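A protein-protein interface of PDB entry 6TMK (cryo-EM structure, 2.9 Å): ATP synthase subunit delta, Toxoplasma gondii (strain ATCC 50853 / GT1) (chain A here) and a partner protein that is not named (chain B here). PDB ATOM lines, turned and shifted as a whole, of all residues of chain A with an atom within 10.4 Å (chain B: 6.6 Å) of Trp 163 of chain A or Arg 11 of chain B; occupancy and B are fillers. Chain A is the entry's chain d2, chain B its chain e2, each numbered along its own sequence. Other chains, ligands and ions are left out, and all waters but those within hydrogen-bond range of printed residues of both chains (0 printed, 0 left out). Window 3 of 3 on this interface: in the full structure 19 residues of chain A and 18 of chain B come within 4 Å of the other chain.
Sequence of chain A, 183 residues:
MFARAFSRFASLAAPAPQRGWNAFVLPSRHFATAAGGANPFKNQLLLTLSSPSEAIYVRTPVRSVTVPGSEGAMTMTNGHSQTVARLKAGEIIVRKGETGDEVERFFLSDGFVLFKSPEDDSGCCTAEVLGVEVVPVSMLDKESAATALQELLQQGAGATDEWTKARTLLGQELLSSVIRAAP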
ATOM      1  N   SER A 109     -22.871   4.760  26.361  1.00  0.00           N
ATOM      2  CA  SER A 109     -23.102   3.406  25.870  1.00  0.00           C
ATOM      3  C   SER A 109     -22.751   2.377  26.937  1.00  0.00           C
ATOM      4  O   SER A 109     -23.618   1.642  27.420  1.00  0.00           O
ATOM      5  CB  SER A 109     -22.287   3.161  24.601  1.00  0.00           C
ATOM      6  OG  SER A 109     -22.196   1.777  24.316  1.00  0.00           O
ATOM      7  N   ASP A 110     -21.479   2.324  27.324  1.00  0.00           N
ATOM      8  CA  ASP A 110     -20.983   1.314  28.244  1.00  0.00           C
ATOM      9  C   ASP A 110     -19.751   1.869  28.941  1.00  0.00           C
ATOM     10  O   ASP A 110     -19.080   2.769  28.430  1.00  0.00           O
ATOM     11  CB  ASP A 110     -20.647   0.008  27.517  1.00  0.00           C
ATOM     12  CG  ASP A 110     -21.883  -0.759  27.095  1.00  0.00           C
ATOM     13  OD1 ASP A 110     -22.878  -0.753  27.850  1.00  0.00           O
ATOM     14  OD2 ASP A 110     -21.865  -1.359  26.000  1.00  0.00           O
ATOM     15  N   VAL A 132     -17.170   4.463  26.915  1.00  0.00           N
ATOM     16  CA  VAL A 132     -16.526   4.130  25.652  1.00  0.00           C
ATOM     17  C   VAL A 132     -17.004   5.048  24.536  1.00  0.00           C
ATOM     18  O   VAL A 132     -16.290   5.241  23.545  1.00  0.00           O
ATOM     19  CB  VAL A 132     -16.783   2.656  25.295  1.00  0.00           C
ATOM     20  CG1 VAL A 132     -15.995   2.259  24.060  1.00  0.00           C
ATOM     21  CG2 VAL A 132     -16.411   1.765  26.465  1.00  0.00           C
ATOM     22  N   LEU A 152     -30.693  -3.796  12.322  1.00  0.00           N
ATOM     23  CA  LEU A 152     -30.251  -4.767  13.315  1.00  0.00           C
ATOM     24  C   LEU A 152     -31.223  -5.934  13.410  1.00  0.00           C
ATOM     25  O   LEU A 152     -30.811  -7.098  13.434  1.00  0.00           O
ATOM     26  CB  LEU A 152     -30.093  -4.082  14.673  1.00  0.00           C
ATOM     27  CG  LEU A 152     -29.535  -4.938  15.809  1.00  0.00           C
ATOM     28  CD1 LEU A 152     -28.020  -4.886  15.835  1.00  0.00           C
ATOM     29  CD2 LEU A 152     -30.101  -4.467  17.135  1.00  0.00           C
ATOM     30  N   GLN A 155     -30.801  -8.103  10.412  1.00  0.00           N
ATOM     31  CA  GLN A 155     -29.615  -8.949  10.448  1.00  0.00           C
ATOM     32  C   GLN A 155     -29.792 -10.088  11.444  1.00  0.00           C
ATOM     33  O   GLN A 155     -29.350 -11.215  11.193  1.00  0.00           O
ATOM     34  CB  GLN A 155     -28.391  -8.105  10.806  1.00  0.00           C
ATOM     35  CG  GLN A 155     -27.062  -8.817  10.630  1.00  0.00           C
ATOM     36  CD  GLN A 155     -26.656  -9.623  11.850  1.00  0.00           C
ATOM     37  OE1 GLN A 155     -27.104  -9.354  12.965  1.00  0.00           O
ATOM     38  NE2 GLN A 155     -25.798 -10.616  11.643  1.00  0.00           N
ATOM     39  N   GLY A 156     -30.437  -9.812  12.578  1.00  0.00           N
ATOM     40  CA  GLY A 156     -30.609 -10.802  13.623  1.00  0.00           C
ATOM     41  C   GLY A 156     -31.793 -11.722  13.443  1.00  0.00           C
ATOM     42  O   GLY A 156     -31.954 -12.660  14.229  1.00  0.00           O
ATOM     43  N   GLY A 158     -32.073 -13.889  11.196  1.00  0.00           N
ATOM     44  CA  GLY A 158     -31.434 -15.169  10.984  1.00  0.00           C
ATOM     45  C   GLY A 158     -30.663 -15.595  12.216  1.00  0.00           C
ATOM     46  O   GLY A 158     -29.431 -15.687  12.191  1.00  0.00           O
ATOM     47  N   ALA A 159     -31.383 -15.852  13.304  1.00  0.00           N
ATOM     48  CA  ALA A 159     -30.773 -16.116  14.604  1.00  0.00           C
ATOM     49  C   ALA A 159     -30.152 -17.505  14.582  1.00  0.00           C
ATOM     50  O   ALA A 159     -30.850 -18.515  14.688  1.00  0.00           O
ATOM     51  CB  ALA A 159     -31.811 -15.992  15.713  1.00  0.00           C
ATOM     52  N   THR A 160     -28.829 -17.557  14.438  1.00  0.00           N
ATOM     53  CA  THR A 160     -28.075 -18.802  14.532  1.00  0.00           C
ATOM     54  C   THR A 160     -27.015 -18.770  15.622  1.00  0.00           C
ATOM     55  O   THR A 160     -26.898 -19.732  16.390  1.00  0.00           O
ATOM     56  CB  THR A 160     -27.436 -19.128  13.168  1.00  0.00           C
ATOM     57  OG1 THR A 160     -26.767 -20.392  13.237  1.00  0.00           O
ATOM     58  CG2 THR A 160     -26.449 -18.044  12.740  1.00  0.00           C
ATOM     59  N   ASP A 161     -26.236 -17.696  15.716  1.00  0.00           N
ATOM     60  CA  ASP A 161     -25.140 -17.624  16.671  1.00  0.00           C
ATOM     61  C   ASP A 161     -25.569 -16.963  17.976  1.00  0.00           C
ATOM     62  O   ASP A 161     -26.397 -16.043  17.998  1.00  0.00           O
ATOM     63  CB  ASP A 161     -23.959 -16.854  16.077  1.00  0.00           C
ATOM     64  CG  ASP A 161     -22.936 -17.765  15.421  1.00  0.00           C
ATOM     65  OD1 ASP A 161     -23.224 -18.969  15.253  1.00  0.00           O
ATOM     66  OD2 ASP A 161     -21.840 -17.276  15.075  1.00  0.00           O
ATOM     67  N   GLU A 162     -24.961 -17.428  19.072  1.00  0.00           N
ATOM     68  CA  GLU A 162     -25.267 -16.869  20.382  1.00  0.00           C
ATOM     69  C   GLU A 162     -24.873 -15.403  20.437  1.00  0.00           C
ATOM     70  O   GLU A 162     -25.609 -14.573  20.983  1.00  0.00           O
ATOM     71  CB  GLU A 162     -24.547 -17.653  21.477  1.00  0.00           C
ATOM     72  CG  GLU A 162     -24.659 -19.162  21.343  1.00  0.00           C
ATOM     73  CD  GLU A 162     -23.471 -19.778  20.628  1.00  0.00           C
ATOM     74  OE1 GLU A 162     -22.680 -19.024  20.023  1.00  0.00           O
ATOM     75  OE2 GLU A 162     -23.330 -21.018  20.670  1.00  0.00           O
ATOM     76  N   TRP A 163     -23.717 -15.064  19.864  1.00  0.00           N
ATOM     77  CA  TRP A 163     -23.265 -13.683  19.922  1.00  0.00           C
ATOM     78  C   TRP A 163     -24.154 -12.799  19.068  1.00  0.00           C
ATOM     79  O   TRP A 163     -24.395 -11.644  19.419  1.00  0.00           O
ATOM     80  CB  TRP A 163     -21.811 -13.575  19.470  1.00  0.00           C
ATOM     81  CG  TRP A 163     -21.328 -12.159  19.358  1.00  0.00           C
ATOM     82  CD1 TRP A 163     -20.636 -11.612  18.319  1.00  0.00           C
ATOM     83  CD2 TRP A 163     -21.515 -11.105  20.313  1.00  0.00           C
ATOM     84  NE1 TRP A 163     -20.374 -10.288  18.567  1.00  0.00           N
ATOM     85  CE2 TRP A 163     -20.903  -9.952  19.785  1.00  0.00           C
ATOM     86  CE3 TRP A 163     -22.134 -11.025  21.564  1.00  0.00           C
ATOM     87  CZ2 TRP A 163     -20.894  -8.737  20.462  1.00  0.00           C
ATOM     88  CZ3 TRP A 163     -22.122  -9.818  22.232  1.00  0.00           C
ATOM     89  CH2 TRP A 163     -21.507  -8.690  21.681  1.00  0.00           C
ATOM     90  N   THR A 164     -24.693 -13.341  17.976  1.00  0.00           N
ATOM     91  CA  THR A 164     -25.572 -12.556  17.121  1.00  0.00           C
ATOM     92  C   THR A 164     -26.895 -12.283  17.826  1.00  0.00           C
ATOM     93  O   THR A 164     -27.390 -11.149  17.821  1.00  0.00           O
ATOM     94  CB  THR A 164     -25.809 -13.286  15.800  1.00  0.00           C
ATOM     95  OG1 THR A 164     -24.554 -13.524  15.151  1.00  0.00           O
ATOM     96  CG2 THR A 164     -26.705 -12.463  14.886  1.00  0.00           C
ATOM     97  N   LYS A 165     -27.483 -13.313  18.437  1.00  0.00           N
ATOM     98  CA  LYS A 165     -28.700 -13.110  19.219  1.00  0.00           C
ATOM     99  C   LYS A 165     -28.475 -12.105  20.345  1.00  0.00           C
ATOM    100  O   LYS A 165     -29.275 -11.180  20.543  1.00  0.00           O
ATOM    101  CB  LYS A 165     -29.195 -14.444  19.775  1.00  0.00           C
ATOM    102  CG  LYS A 165     -29.541 -15.458  18.703  1.00  0.00           C
ATOM    103  CD  LYS A 165     -29.988 -16.774  19.310  1.00  0.00           C
ATOM    104  CE  LYS A 165     -28.813 -17.569  19.842  1.00  0.00           C
ATOM    105  NZ  LYS A 165     -29.102 -19.028  19.888  1.00  0.00           N
ATOM    106  N   ALA A 166     -27.398 -12.288  21.114  1.00  0.00           N
ATOM    107  CA  ALA A 166     -27.109 -11.379  22.216  1.00  0.00           C
ATOM    108  C   ALA A 166     -26.916  -9.953  21.720  1.00  0.00           C
ATOM    109  O   ALA A 166     -27.410  -9.001  22.336  1.00  0.00           O
ATOM    110  CB  ALA A 166     -25.873 -11.855  22.975  1.00  0.00           C
ATOM    111  N   ARG A 167     -26.182  -9.782  20.619  1.00  0.00           N
ATOM    112  CA  ARG A 167     -25.948  -8.450  20.080  1.00  0.00           C
ATOM    113  C   ARG A 167     -27.247  -7.820  19.606  1.00  0.00           C
ATOM    114  O   ARG A 167     -27.464  -6.620  19.793  1.00  0.00           O
ATOM    115  CB  ARG A 167     -24.952  -8.529  18.928  1.00  0.00           C
ATOM    116  CG  ARG A 167     -24.396  -7.191  18.492  1.00  0.00           C
ATOM    117  CD  ARG A 167     -23.210  -7.376  17.573  1.00  0.00           C
ATOM    118  NE  ARG A 167     -23.640  -7.841  16.259  1.00  0.00           N
ATOM    119  CZ  ARG A 167     -24.202  -7.064  15.340  1.00  0.00           C
ATOM    120  NH1 ARG A 167     -24.409  -5.778  15.585  1.00  0.00           N
ATOM    121  NH2 ARG A 167     -24.565  -7.577  14.173  1.00  0.00           N
ATOM    122  N   THR A 168     -28.129  -8.615  19.002  1.00  0.00           N
ATOM    123  CA  THR A 168     -29.430  -8.098  18.593  1.00  0.00           C
ATOM    124  C   THR A 168     -30.224  -7.612  19.798  1.00  0.00           C
ATOM    125  O   THR A 168     -30.793  -6.514  19.785  1.00  0.00           O
ATOM    126  CB  THR A 168     -30.204  -9.179  17.840  1.00  0.00           C
ATOM    127  OG1 THR A 168     -29.521  -9.500  16.622  1.00  0.00           O
ATOM    128  CG2 THR A 168     -31.614  -8.708  17.517  1.00  0.00           C
ATOM    129  N   LEU A 169     -30.251  -8.411  20.866  1.00  0.00           N
ATOM    130  CA  LEU A 169     -31.012  -8.020  22.050  1.00  0.00           C
ATOM    131  C   LEU A 169     -30.426  -6.770  22.698  1.00  0.00           C
ATOM    132  O   LEU A 169     -31.165  -5.855  23.088  1.00  0.00           O
ATOM    133  CB  LEU A 169     -31.045  -9.175  23.047  1.00  0.00           C
ATOM    134  CG  LEU A 169     -32.091 -10.254  22.765  1.00  0.00           C
ATOM    135  CD1 LEU A 169     -31.747 -11.533  23.506  1.00  0.00           C
ATOM    136  CD2 LEU A 169     -33.484  -9.773  23.145  1.00  0.00           C
ATOM    137  N   LEU A 170     -29.101  -6.704  22.811  1.00  0.00           N
ATOM    138  CA  LEU A 170     -28.479  -5.554  23.454  1.00  0.00           C
ATOM    139  C   LEU A 170     -28.618  -4.301  22.595  1.00  0.00           C
ATOM    140  O   LEU A 170     -28.773  -3.194  23.125  1.00  0.00           O
ATOM    141  CB  LEU A 170     -27.014  -5.859  23.746  1.00  0.00           C
ATOM    142  CG  LEU A 170     -26.819  -6.877  24.872  1.00  0.00           C
ATOM    143  CD1 LEU A 170     -25.573  -7.707  24.649  1.00  0.00           C
ATOM    144  CD2 LEU A 170     -26.765  -6.185  26.219  1.00  0.00           C
ATOM    145  N   GLY A 171     -28.553  -4.451  21.272  1.00  0.00           N
ATOM    146  CA  GLY A 171     -28.835  -3.329  20.400  1.00  0.00           C
ATOM    147  C   GLY A 171     -30.260  -2.837  20.544  1.00  0.00           C
ATOM    148  O   GLY A 171     -30.513  -1.633  20.542  1.00  0.00           O
ATOM    149  N   MET B   1     -24.274 -11.845  30.025  1.00  0.00           N
ATOM    150  CA  MET B   1     -24.736 -12.254  28.669  1.00  0.00           C
ATOM    151  C   MET B   1     -23.572 -12.538  27.729  1.00  0.00           C
ATOM    152  O   MET B   1     -23.776 -12.988  26.602  1.00  0.00           O
ATOM    153  CB  MET B   1     -25.628 -11.174  28.060  1.00  0.00           C
ATOM    154  CG  MET B   1     -26.528 -10.470  29.051  1.00  0.00           C
ATOM    155  SD  MET B   1     -27.800  -9.488  28.233  1.00  0.00           S
ATOM    156  CE  MET B   1     -28.776 -10.773  27.460  1.00  0.00           C
ATOM    157  N   TRP B   2     -22.353 -12.278  28.187  1.00  0.00           N
ATOM    158  CA  TRP B   2     -21.186 -12.355  27.320  1.00  0.00           C
ATOM    159  C   TRP B   2     -20.217 -13.441  27.747  1.00  0.00           C
ATOM    160  O   TRP B   2     -19.651 -14.127  26.896  1.00  0.00           O
ATOM    161  CB  TRP B   2     -20.460 -11.006  27.286  1.00  0.00           C
ATOM    162  CG  TRP B   2     -21.389  -9.904  26.965  1.00  0.00           C
ATOM    163  CD1 TRP B   2     -21.812  -9.519  25.733  1.00  0.00           C
ATOM    164  CD2 TRP B   2     -22.011  -9.021  27.903  1.00  0.00           C
ATOM    165  NE1 TRP B   2     -22.675  -8.456  25.842  1.00  0.00           N
ATOM    166  CE2 TRP B   2     -22.810  -8.129  27.166  1.00  0.00           C
ATOM    167  CE3 TRP B   2     -21.969  -8.899  29.293  1.00  0.00           C
ATOM    168  CZ2 TRP B   2     -23.566  -7.131  27.776  1.00  0.00           C
ATOM    169  CZ3 TRP B   2     -22.721  -7.909  29.895  1.00  0.00           C
ATOM    170  CH2 TRP B   2     -23.506  -7.038  29.138  1.00  0.00           C
ATOM    171  N   SER B   5     -21.996 -16.392  26.369  1.00  0.00           N
ATOM    172  CA  SER B   5     -21.860 -16.483  24.923  1.00  0.00           C
ATOM    173  C   SER B   5     -20.411 -16.597  24.464  1.00  0.00           C
ATOM    174  O   SER B   5     -20.170 -16.709  23.258  1.00  0.00           O
ATOM    175  CB  SER B   5     -22.511 -15.263  24.266  1.00  0.00           C
ATOM    176  OG  SER B   5     -23.850 -15.111  24.697  1.00  0.00           O
ATOM    177  N   GLY B   6     -19.452 -16.573  25.384  1.00  0.00           N
ATOM    178  CA  GLY B   6     -18.049 -16.602  25.021  1.00  0.00           C
ATOM    179  C   GLY B   6     -17.630 -15.325  24.328  1.00  0.00           C
ATOM    180  O   GLY B   6     -17.073 -15.348  23.226  1.00  0.00           O
ATOM    181  N   VAL B   7     -17.903 -14.200  24.981  1.00  0.00           N
ATOM    182  CA  VAL B   7     -17.664 -12.876  24.425  1.00  0.00           C
ATOM    183  C   VAL B   7     -17.086 -11.999  25.525  1.00  0.00           C
ATOM    184  O   VAL B   7     -17.419 -12.149  26.704  1.00  0.00           O
ATOM    185  CB  VAL B   7     -18.949 -12.267  23.833  1.00  0.00           C
ATOM    186  CG1 VAL B   7     -18.685 -10.875  23.307  1.00  0.00           C
ATOM    187  CG2 VAL B   7     -19.480 -13.162  22.728  1.00  0.00           C
ATOM    188  N   SER B   8     -16.212 -11.081  25.133  1.00  0.00           N
ATOM    189  CA  SER B   8     -15.556 -10.188  26.073  1.00  0.00           C
ATOM    190  C   SER B   8     -16.308  -8.872  26.222  1.00  0.00           C
ATOM    191  O   SER B   8     -17.022  -8.423  25.317  1.00  0.00           O
ATOM    192  CB  SER B   8     -14.123  -9.908  25.628  1.00  0.00           C
ATOM    193  OG  SER B   8     -14.069  -9.630  24.240  1.00  0.00           O
ATOM    194  N   PHE B   9     -16.119  -8.244  27.385  1.00  0.00           N
ATOM    195  CA  PHE B   9     -16.760  -6.964  27.646  1.00  0.00           C
ATOM    196  C   PHE B   9     -16.226  -5.885  26.722  1.00  0.00           C
ATOM    197  O   PHE B   9     -16.971  -4.980  26.339  1.00  0.00           O
ATOM    198  CB  PHE B   9     -16.563  -6.571  29.109  1.00  0.00           C
ATOM    199  CG  PHE B   9     -17.233  -5.283  29.486  1.00  0.00           C
ATOM    200  CD1 PHE B   9     -18.609  -5.209  29.593  1.00  0.00           C
ATOM    201  CD2 PHE B   9     -16.484  -4.155  29.758  1.00  0.00           C
ATOM    202  CE1 PHE B   9     -19.225  -4.029  29.943  1.00  0.00           C
ATOM    203  CE2 PHE B   9     -17.096  -2.971  30.110  1.00  0.00           C
ATOM    204  CZ  PHE B   9     -18.468  -2.909  30.206  1.00  0.00           C
ATOM    205  N   THR B  10     -14.956  -5.975  26.328  1.00  0.00           N
ATOM    206  CA  THR B  10     -14.414  -4.985  25.408  1.00  0.00           C
ATOM    207  C   THR B  10     -15.055  -5.130  24.035  1.00  0.00           C
ATOM    208  O   THR B  10     -15.408  -4.133  23.396  1.00  0.00           O
ATOM    209  CB  THR B  10     -12.899  -5.138  25.311  1.00  0.00           C
ATOM    210  OG1 THR B  10     -12.576  -6.478  24.923  1.00  0.00           O
ATOM    211  CG2 THR B  10     -12.251  -4.832  26.643  1.00  0.00           C
ATOM    212  N   ARG B  11     -15.227  -6.371  23.581  1.00  0.00           N
ATOM    213  CA  ARG B  11     -15.917  -6.621  22.322  1.00  0.00           C
ATOM    214  C   ARG B  11     -17.340  -6.080  22.367  1.00  0.00           C
ATOM    215  O   ARG B  11     -17.787  -5.394  21.441  1.00  0.00           O
ATOM    216  CB  ARG B  11     -15.924  -8.118  22.021  1.00  0.00           C
ATOM    217  CG  ARG B  11     -16.432  -8.464  20.637  1.00  0.00           C
ATOM    218  CD  ARG B  11     -16.200  -9.924  20.312  1.00  0.00           C
ATOM    219  NE  ARG B  11     -16.796 -10.298  19.033  1.00  0.00           N
ATOM    220  CZ  ARG B  11     -16.837 -11.538  18.562  1.00  0.00           C
ATOM    221  NH1 ARG B  11     -16.314 -12.534  19.263  1.00  0.00           N
ATOM    222  NH2 ARG B  11     -17.399 -11.784  17.390  1.00  0.00           N
ATOM    223  N   TYR B  12     -18.070  -6.390  23.439  1.00  0.00           N
ATOM    224  CA  TYR B  12     -19.442  -5.906  23.565  1.00  0.00           C
ATOM    225  C   TYR B  12     -19.492  -4.382  23.580  1.00  0.00           C
ATOM    226  O   TYR B  12     -20.314  -3.772  22.883  1.00  0.00           O
ATOM    227  CB  TYR B  12     -20.083  -6.491  24.823  1.00  0.00           C
ATOM    228  CG  TYR B  12     -21.127  -5.611  25.467  1.00  0.00           C
ATOM    229  CD1 TYR B  12     -22.414  -5.544  24.959  1.00  0.00           C
ATOM    230  CD2 TYR B  12     -20.837  -4.883  26.609  1.00  0.00           C
ATOM    231  CE1 TYR B  12     -23.372  -4.751  25.550  1.00  0.00           C
ATOM    232  CE2 TYR B  12     -21.790  -4.091  27.209  1.00  0.00           C
ATOM    233  CZ  TYR B  12     -23.055  -4.027  26.676  1.00  0.00           C
ATOM    234  OH  TYR B  12     -24.009  -3.238  27.274  1.00  0.00           O
ATOM    235  N   ALA B  13     -18.599  -3.748  24.340  1.00  0.00           N
ATOM    236  CA  ALA B  13     -18.610  -2.296  24.445  1.00  0.00           C
ATOM    237  C   ALA B  13     -18.299  -1.650  23.105  1.00  0.00           C
ATOM    238  O   ALA B  13     -18.950  -0.676  22.713  1.00  0.00           O
ATOM    239  CB  ALA B  13     -17.609  -1.848  25.503  1.00  0.00           C
ATOM    240  N   SER B  14     -17.316  -2.182  22.380  1.00  0.00           N
ATOM    241  CA  SER B  14     -16.971  -1.622  21.080  1.00  0.00           C
ATOM    242  C   SER B  14     -18.117  -1.800  20.093  1.00  0.00           C
ATOM    243  O   SER B  14     -18.501  -0.858  19.390  1.00  0.00           O
ATOM    244  CB  SER B  14     -15.699  -2.278  20.554  1.00  0.00           C
ATOM    245  OG  SER B  14     -14.661  -2.211  21.515  1.00  0.00           O
ATOM    246  N   GLU B  15     -18.658  -3.017  20.006  1.00  0.00           N
ATOM    247  CA  GLU B  15     -19.718  -3.297  19.049  1.00  0.00           C
ATOM    248  C   GLU B  15     -21.003  -2.543  19.375  1.00  0.00           C
ATOM    249  O   GLU B  15     -21.839  -2.364  18.483  1.00  0.00           O
ATOM    250  CB  GLU B  15     -19.977  -4.800  18.999  1.00  0.00           C
ATOM    251  CG  GLU B  15     -18.824  -5.576  18.374  1.00  0.00           C
ATOM    252  CD  GLU B  15     -19.179  -7.012  18.051  1.00  0.00           C
ATOM    253  OE1 GLU B  15     -20.360  -7.285  17.760  1.00  0.00           O
ATOM    254  OE2 GLU B  15     -18.271  -7.869  18.087  1.00  0.00           O
ATOM    255  N   MET B  16     -21.184  -2.101  20.621  1.00  0.00           N
ATOM    256  CA  MET B  16     -22.343  -1.283  20.957  1.00  0.00           C
ATOM    257  C   MET B  16     -22.076   0.201  20.745  1.00  0.00           C
ATOM    258  O   MET B  16     -22.980   0.944  20.333  1.00  0.00           O
ATOM    259  CB  MET B  16     -22.750  -1.521  22.413  1.00  0.00           C
ATOM    260  CG  MET B  16     -23.413  -2.865  22.670  1.00  0.00           C
ATOM    261  SD  MET B  16     -24.933  -3.146  21.743  1.00  0.00           S
ATOM    262  CE  MET B  16     -25.920  -1.755  22.280  1.00  0.00           C
ATOM    263  N   ILE B  59     -14.458  -3.695  12.787  1.00  0.00           N
ATOM    264  CA  ILE B  59     -14.369  -4.148  14.170  1.00  0.00           C
ATOM    265  C   ILE B  59     -14.877  -5.578  14.292  1.00  0.00           C
ATOM    266  O   ILE B  59     -14.283  -6.407  14.993  1.00  0.00           O
ATOM    267  CB  ILE B  59     -15.137  -3.183  15.089  1.00  0.00           C
ATOM    268  CG1 ILE B  59     -14.824  -3.474  16.557  1.00  0.00           C
ATOM    269  CG2 ILE B  59     -16.633  -3.262  14.828  1.00  0.00           C
ATOM    270  CD1 ILE B  59     -13.433  -3.074  16.964  1.00  0.00           C
ATOM    271  N   LYS B  60     -15.979  -5.893  13.611  1.00  0.00           N
ATOM    272  CA  LYS B  60     -16.602  -7.196  13.800  1.00  0.00           C
ATOM    273  C   LYS B  60     -15.737  -8.297  13.209  1.00  0.00           C
ATOM    274  O   LYS B  60     -15.548  -9.346  13.833  1.00  0.00           O
ATOM    275  CB  LYS B  60     -17.994  -7.212  13.172  1.00  0.00           C
ATOM    276  CG  LYS B  60     -18.947  -6.178  13.746  1.00  0.00           C
ATOM    277  CD  LYS B  60     -20.215  -6.077  12.918  1.00  0.00           C
ATOM    278  CE  LYS B  60     -21.238  -5.167  13.575  1.00  0.00           C
ATOM    279  NZ  LYS B  60     -22.243  -4.663  12.600  1.00  0.00           N
ATOM    280  N   PHE B  63     -12.644  -8.784  15.471  1.00  0.00           N
ATOM    281  CA  PHE B  63     -12.880  -9.590  16.662  1.00  0.00           C
ATOM    282  C   PHE B  63     -13.209 -11.029  16.296  1.00  0.00           C
ATOM    283  O   PHE B  63     -12.904 -11.946  17.067  1.00  0.00           O
ATOM    284  CB  PHE B  63     -14.007  -8.983  17.494  1.00  0.00           C
ATOM    285  CG  PHE B  63     -13.556  -7.888  18.411  1.00  0.00           C
ATOM    286  CD1 PHE B  63     -14.079  -6.616  18.296  1.00  0.00           C
ATOM    287  CD2 PHE B  63     -12.622  -8.137  19.400  1.00  0.00           C
ATOM    288  CE1 PHE B  63     -13.670  -5.609  19.141  1.00  0.00           C
ATOM    289  CE2 PHE B  63     -12.210  -7.134  20.246  1.00  0.00           C
ATOM    290  CZ  PHE B  63     -12.732  -5.868  20.116  1.00  0.00           C
ATOM    291  N   GLU B  64     -13.823 -11.245  15.133  1.00  0.00           N
ATOM    292  CA  GLU B  64     -14.193 -12.592  14.720  1.00  0.00           C
ATOM    293  C   GLU B  64     -12.958 -13.391  14.331  1.00  0.00           C
ATOM    294  O   GLU B  64     -12.672 -14.443  14.913  1.00  0.00           O
ATOM    295  CB  GLU B  64     -15.185 -12.524  13.558  1.00  0.00           C
ATOM    296  CG  GLU B  64     -15.537 -13.874  12.957  1.00  0.00           C
ATOM    297  CD  GLU B  64     -15.981 -14.882  13.998  1.00  0.00           C
ATOM    298  OE1 GLU B  64     -16.608 -14.472  14.997  1.00  0.00           O
ATOM    299  OE2 GLU B  64     -15.702 -16.087  13.818  1.00  0.00           O
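Of the printed residues of chain B, Ser 109 of chain A touches Met 16 (3.8 Å).
Printed residues of chain B within 4 Å of Asp 110 of chain A: Tyr 12, Ala 13 and Met 16.
Trp 163 of chain A touches just these residues of chain B: Trp 2, Val 7, Arg 11, Tyr 12 and Glu 15.
Of the printed residues of chain B, Gly 171 of chain A touches Met 16.
Thr 10 of chain B touches none of the printed residues of chain A.
Of chain A, only Trp 163 comes within 4 Å of Arg 11 of chain B.
Of chain A, only Asp 110 (3.7 Å) and Val 132 (3.9 Å) come within 4 Å of Ala 13 of chain B.
Of the printed residues of chain A, Lys 60 of chain B touches Arg 167.
The nearest residue of chain B that does not touch Trp 163 of chain A is Ser 5 of chain B (4.6 Å).
Of the 20 printed residues of chain A, 7 touch a printed residue of chain B.
Hydrophobic or aromatic side chains of chain A that line the printed part of chain B: Val 132, Trp 163 and Leu 170.
Of the 18 printed residues of chain B, 8 touch a printed residue of chain A.
Hydrophobic or aromatic side chains of chain B that line the printed part of chain A: Trp 2, Val 7, Tyr 12, Ala 13 and Met 16.
The side-chain hydroxyl (OH) of Tyr 12 of chain B is in hydrogen-bond range of the side-chain carboxylate (OD1) of Asp 110 of chain A.
NE1 of Trp 163 of chain A is in hydrogen-bond range of OE1 of Glu 15 of chain B (3.1 Å).
The guanidinium group of Arg 167 of chain A is in salt-bridge range of the side-chain carboxylate of Glu 15 of chain B, at 3.6 Å.
The backbone NH of Val 132 of chain A sits at hydrogen-bond distance from the backbone carbonyl oxygen of Asp 110 of chain A (3.0 Å).
The side-chain amide oxygen of Gln 155 of chain A lies within hydrogen-bond range of the guanidinium group of Arg 167 of chain A (3.3 Å).
The backbone NH of Val 7 of chain B sits at hydrogen-bond distance from the backbone carbonyl oxygen of Trp 2 of chain B (2.6 Å).
The guanidinium group of Arg 11 of chain B is in salt-bridge range of the side-chain carboxylate of Glu 15 of chain B, at 3.0 Å.
The guanidinium group (NH2) of Arg 11 of chain B is in salt-bridge range of the side-chain carboxylate (OE1) of Glu 64 of chain B.
Among the printed residues, merely in contact across the chains: Ser 109 of chain A with Met 16 of chain B (3.8 Å), Asp 110 of chain A with Ala 13 of chain B (3.7 Å), Asp 110 of chain A with Met 16 of chain B (3.7 Å), Val 132 of chain A with Ala 13 of chain B (3.9 Å), Trp 163 of chain A with Trp 2 of chain B (3.5 Å), Trp 163 of chain A with Val 7 of chain B (3.6 Å), Trp 163 of chain A with Arg 11 of chain B (3.4 Å), Trp 163 of chain A with Tyr 12 of chain B (3.9 Å), Arg 167 of chain A with Lys 60 of chain B (3.8 Å), Leu 170 of chain A with Trp 2 of chain B (3.2 Å), Leu 170 of chain A with Tyr 12 of chain B (3.7 Å), Leu 170 of chain A with Met 16 of chain B (3.3 Å) and Gly 171 of chain A with Met 16 of chain B (3.8 Å).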
